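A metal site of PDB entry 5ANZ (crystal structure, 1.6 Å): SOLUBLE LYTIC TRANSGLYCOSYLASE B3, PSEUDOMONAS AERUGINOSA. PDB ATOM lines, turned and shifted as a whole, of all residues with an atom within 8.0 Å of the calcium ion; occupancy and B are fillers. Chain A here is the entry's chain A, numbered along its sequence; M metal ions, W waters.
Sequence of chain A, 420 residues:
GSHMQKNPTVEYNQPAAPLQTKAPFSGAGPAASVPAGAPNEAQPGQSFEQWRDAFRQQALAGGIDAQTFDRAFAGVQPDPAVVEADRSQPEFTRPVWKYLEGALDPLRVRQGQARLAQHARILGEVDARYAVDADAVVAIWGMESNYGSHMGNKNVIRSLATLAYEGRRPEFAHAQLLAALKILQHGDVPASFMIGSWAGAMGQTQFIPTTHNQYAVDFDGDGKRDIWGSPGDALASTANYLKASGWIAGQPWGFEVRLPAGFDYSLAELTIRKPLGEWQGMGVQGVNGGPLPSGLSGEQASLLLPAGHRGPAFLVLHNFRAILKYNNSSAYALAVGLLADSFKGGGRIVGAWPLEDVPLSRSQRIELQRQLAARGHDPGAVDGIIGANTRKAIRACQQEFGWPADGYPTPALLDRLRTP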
ATOM      1  N   ASP A 188     -26.567  16.399  28.288  1.00  0.00           N
ATOM      2  CA  ASP A 188     -26.254  16.665  26.878  1.00  0.00           C
ATOM      3  C   ASP A 188     -27.413  17.353  26.141  1.00  0.00           C
ATOM      4  O   ASP A 188     -27.193  18.127  25.197  1.00  0.00           O
ATOM      5  CB  ASP A 188     -25.904  15.372  26.122  1.00  0.00           C
ATOM      6  CG  ASP A 188     -24.518  14.816  26.469  1.00  0.00           C
ATOM      7  OD1 ASP A 188     -23.592  15.583  26.824  1.00  0.00           O
ATOM      8  OD2 ASP A 188     -24.352  13.578  26.343  1.00  0.00           O
ATOM      9  N   VAL A 217     -18.994  13.384  20.650  1.00  0.00           N
ATOM     10  CA  VAL A 217     -17.944  14.345  20.924  1.00  0.00           C
ATOM     11  C   VAL A 217     -18.507  15.698  21.313  1.00  0.00           C
ATOM     12  O   VAL A 217     -19.512  16.125  20.730  1.00  0.00           O
ATOM     13  CB  VAL A 217     -17.049  14.527  19.676  1.00  0.00           C
ATOM     14  CG1 VAL A 217     -16.087  15.680  19.859  1.00  0.00           C
ATOM     15  CG2 VAL A 217     -16.302  13.227  19.371  1.00  0.00           C
ATOM     16  N   ASP A 218     -17.880  16.383  22.264  1.00  0.00           N
ATOM     17  CA  ASP A 218     -18.156  17.796  22.525  1.00  0.00           C
ATOM     18  C   ASP A 218     -17.144  18.659  21.784  1.00  0.00           C
ATOM     19  O   ASP A 218     -16.026  18.902  22.277  1.00  0.00           O
ATOM     20  CB  ASP A 218     -18.105  18.082  24.032  1.00  0.00           C
ATOM     21  CG  ASP A 218     -18.295  19.546  24.355  1.00  0.00           C
ATOM     22  OD1 ASP A 218     -18.790  20.298  23.483  1.00  0.00           O
ATOM     23  OD2 ASP A 218     -17.950  19.953  25.491  1.00  0.00           O
ATOM     24  N   PHE A 219     -17.523  19.111  20.590  1.00  0.00           N
ATOM     25  CA  PHE A 219     -16.623  19.838  19.724  1.00  0.00           C
ATOM     26  C   PHE A 219     -16.256  21.201  20.265  1.00  0.00           C
ATOM     27  O   PHE A 219     -15.100  21.603  20.216  1.00  0.00           O
ATOM     28  CB  PHE A 219     -17.229  20.004  18.322  1.00  0.00           C
ATOM     29  CG  PHE A 219     -16.351  20.771  17.375  1.00  0.00           C
ATOM     30  CD1 PHE A 219     -15.236  20.176  16.814  1.00  0.00           C
ATOM     31  CD2 PHE A 219     -16.645  22.089  17.034  1.00  0.00           C
ATOM     32  CE1 PHE A 219     -14.416  20.884  15.942  1.00  0.00           C
ATOM     33  CE2 PHE A 219     -15.825  22.797  16.162  1.00  0.00           C
ATOM     34  CZ  PHE A 219     -14.720  22.184  15.608  1.00  0.00           C
ATOM     35  N   ASP A 220     -17.239  21.921  20.789  1.00  0.00           N
ATOM     36  CA  ASP A 220     -17.015  23.322  21.161  1.00  0.00           C
ATOM     37  C   ASP A 220     -16.582  23.511  22.609  1.00  0.00           C
ATOM     38  O   ASP A 220     -16.127  24.582  22.981  1.00  0.00           O
ATOM     39  CB  ASP A 220     -18.265  24.150  20.880  1.00  0.00           C
ATOM     40  CG  ASP A 220     -19.432  23.747  21.751  1.00  0.00           C
ATOM     41  OD1 ASP A 220     -19.943  22.624  21.589  1.00  0.00           O
ATOM     42  OD2 ASP A 220     -19.846  24.560  22.609  1.00  0.00           O
ATOM     43  N   GLY A 221     -16.727  22.469  23.431  1.00  0.00           N
ATOM     44  CA  GLY A 221     -16.231  22.500  24.797  1.00  0.00           C
ATOM     45  C   GLY A 221     -17.169  23.035  25.863  1.00  0.00           C
ATOM     46  O   GLY A 221     -16.751  23.312  26.980  1.00  0.00           O
ATOM     47  N   ASP A 222     -18.449  23.158  25.537  1.00  0.00           N
ATOM     48  CA  ASP A 222     -19.414  23.667  26.510  1.00  0.00           C
ATOM     49  C   ASP A 222     -19.856  22.588  27.508  1.00  0.00           C
ATOM     50  O   ASP A 222     -20.638  22.861  28.410  1.00  0.00           O
ATOM     51  CB  ASP A 222     -20.617  24.285  25.806  1.00  0.00           C
ATOM     52  CG  ASP A 222     -21.455  23.278  25.026  1.00  0.00           C
ATOM     53  OD1 ASP A 222     -20.964  22.164  24.723  1.00  0.00           O
ATOM     54  OD2 ASP A 222     -22.611  23.604  24.690  1.00  0.00           O
ATOM     55  N   GLY A 223     -19.307  21.379  27.362  1.00  0.00           N
ATOM     56  CA  GLY A 223     -19.610  20.278  28.266  1.00  0.00           C
ATOM     57  C   GLY A 223     -20.768  19.421  27.817  1.00  0.00           C
ATOM     58  O   GLY A 223     -21.091  18.410  28.447  1.00  0.00           O
ATOM     59  N   LYS A 224     -21.391  19.801  26.720  1.00  0.00           N
ATOM     60  CA  LYS A 224     -22.492  19.019  26.167  1.00  0.00           C
ATOM     61  C   LYS A 224     -22.109  18.374  24.841  1.00  0.00           C
ATOM     62  O   LYS A 224     -21.535  19.018  23.965  1.00  0.00           O
ATOM     63  CB  LYS A 224     -23.724  19.911  25.957  1.00  0.00           C
ATOM     64  CG  LYS A 224     -24.268  20.522  27.236  1.00  0.00           C
ATOM     65  CD  LYS A 224     -25.625  21.158  27.003  1.00  0.00           C
ATOM     66  CE  LYS A 224     -25.514  22.367  26.094  1.00  0.00           C
ATOM     67  NZ  LYS A 224     -26.802  23.109  26.019  1.00  0.00           N
ATOM     68  N   ARG A 225     -22.413  17.083  24.729  1.00  0.00           N
ATOM     69  CA  ARG A 225     -22.305  16.371  23.453  1.00  0.00           C
ATOM     70  C   ARG A 225     -23.663  16.448  22.776  1.00  0.00           C
ATOM     71  O   ARG A 225     -24.454  15.510  22.827  1.00  0.00           O
ATOM     72  CB  ARG A 225     -21.857  14.932  23.682  1.00  0.00           C
ATOM     73  CG  ARG A 225     -20.492  14.862  24.360  1.00  0.00           C
ATOM     74  CD  ARG A 225     -19.914  13.450  24.293  1.00  0.00           C
ATOM     75  NE  ARG A 225     -20.454  12.579  25.335  1.00  0.00           N
ATOM     76  CZ  ARG A 225     -20.248  11.264  25.413  1.00  0.00           C
ATOM     77  NH1 ARG A 225     -19.502  10.645  24.498  1.00  0.00           N
ATOM     78  NH2 ARG A 225     -20.781  10.574  26.407  1.00  0.00           N
ATOM     79  N   ASP A 226     -23.937  17.588  22.165  1.00  0.00           N
ATOM     80  CA  ASP A 226     -25.269  17.887  21.639  1.00  0.00           C
ATOM     81  C   ASP A 226     -25.402  17.554  20.162  1.00  0.00           C
ATOM     82  O   ASP A 226     -25.202  18.417  19.300  1.00  0.00           O
ATOM     83  CB  ASP A 226     -25.579  19.363  21.867  1.00  0.00           C
ATOM     84  CG  ASP A 226     -26.908  19.777  21.266  1.00  0.00           C
ATOM     85  OD1 ASP A 226     -27.742  18.898  20.972  1.00  0.00           O
ATOM     86  OD2 ASP A 226     -27.122  21.005  21.098  1.00  0.00           O
ATOM     87  N   ILE A 227     -25.758  16.310  19.874  1.00  0.00           N
ATOM     88  CA  ILE A 227     -25.884  15.865  18.494  1.00  0.00           C
ATOM     89  C   ILE A 227     -27.249  16.228  17.935  1.00  0.00           C
ATOM     90  O   ILE A 227     -27.579  15.848  16.820  1.00  0.00           O
ATOM     91  CB  ILE A 227     -25.676  14.346  18.337  1.00  0.00           C
ATOM     92  CG1 ILE A 227     -26.697  13.586  19.188  1.00  0.00           C
ATOM     93  CG2 ILE A 227     -24.252  13.947  18.761  1.00  0.00           C
ATOM     94  CD1 ILE A 227     -26.689  12.060  18.945  1.00  0.00           C
ATOM     95  N   SER A 230     -26.251  21.045  17.773  1.00  0.00           N
ATOM     96  CA  SER A 230     -24.935  21.597  17.463  1.00  0.00           C
ATOM     97  C   SER A 230     -24.293  20.942  16.243  1.00  0.00           C
ATOM     98  O   SER A 230     -23.876  19.796  16.332  1.00  0.00           O
ATOM     99  CB  SER A 230     -23.991  21.414  18.644  1.00  0.00           C
ATOM    100  OG  SER A 230     -22.653  21.679  18.245  1.00  0.00           O
ATOM    101  N   GLY A 232     -21.375  21.388  15.056  1.00  0.00           N
ATOM    102  CA  GLY A 232     -20.007  21.047  15.430  1.00  0.00           C
ATOM    103  C   GLY A 232     -19.941  19.713  16.143  1.00  0.00           C
ATOM    104  O   GLY A 232     -19.179  18.827  15.748  1.00  0.00           O
ATOM    105  N   ASP A 233     -20.726  19.570  17.207  1.00  0.00           N
ATOM    106  CA  ASP A 233     -20.758  18.291  17.946  1.00  0.00           C
ATOM    107  C   ASP A 233     -21.173  17.150  17.033  1.00  0.00           C
ATOM    108  O   ASP A 233     -20.620  16.055  17.075  1.00  0.00           O
ATOM    109  CB  ASP A 233     -21.715  18.342  19.139  1.00  0.00           C
ATOM    110  CG  ASP A 233     -21.276  19.307  20.244  1.00  0.00           C
ATOM    111  OD1 ASP A 233     -20.147  19.876  20.238  1.00  0.00           O
ATOM    112  OD2 ASP A 233     -22.108  19.473  21.174  1.00  0.00           O
ATOM    113  N   ALA A 234     -22.185  17.384  16.200  1.00  0.00           N
ATOM    114  CA  ALA A 234     -22.668  16.338  15.307  1.00  0.00           C
ATOM    115  C   ALA A 234     -21.609  15.891  14.319  1.00  0.00           C
ATOM    116  O   ALA A 234     -21.394  14.706  14.131  1.00  0.00           O
ATOM    117  CB  ALA A 234     -23.913  16.817  14.541  1.00  0.00           C
HETATM  118 CA    CA M   1     -20.952  20.859  22.734  1.00  0.00          CA
HETATM  119  O   HOH W   1     -23.007  22.008  22.557  1.00  0.00           O
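The side-chain carboxylate (OD2) of Asp 218 lies close to the backbone NH (N) of Gly 221, 3.5 Å away. The side-chain carboxylate (OD2) of Asp 218 lies within hydrogen-bond range of the backbone NH (N) of Gly 223, 2.7 Å away. The side-chain carboxylate of Asp 233 sits close to the backbone NH of Phe 219, 2.8 Å away. The backbone NH (N) of Asp 226 lies close to the side-chain carboxylate (OD2) of Asp 233 (2.8 Å). N of Asp 233 is in hydrogen-bond range of OG of Ser 230, at 3.0 Å.
O of Lys 224 binds the calcium ion. The calcium ion is bound by the side-chain carboxylate (OD1) of Asp 220 (2.3 Å). OD1 of Asp 218 is bound to the calcium ion, at 2.4 Å. Water W1 binds the calcium ion. OD1 of Asp 222 binds the calcium ion (2.4 Å). The side-chain carboxylate (OD2) of Asp 233 is bound to the calcium ion (2.4 Å). OD1 of Asp 233 is bound to the calcium ion, at 2.8 Å. The calcium ion has seven donor atoms within binding distance.
Within 4 Å of the calcium ion: Asp 218, Asp 220, Asp 222, Lys 224 and Asp 233. The nearest printed residue that does not touch the calcium ion is Phe 219 (4.4 Å).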
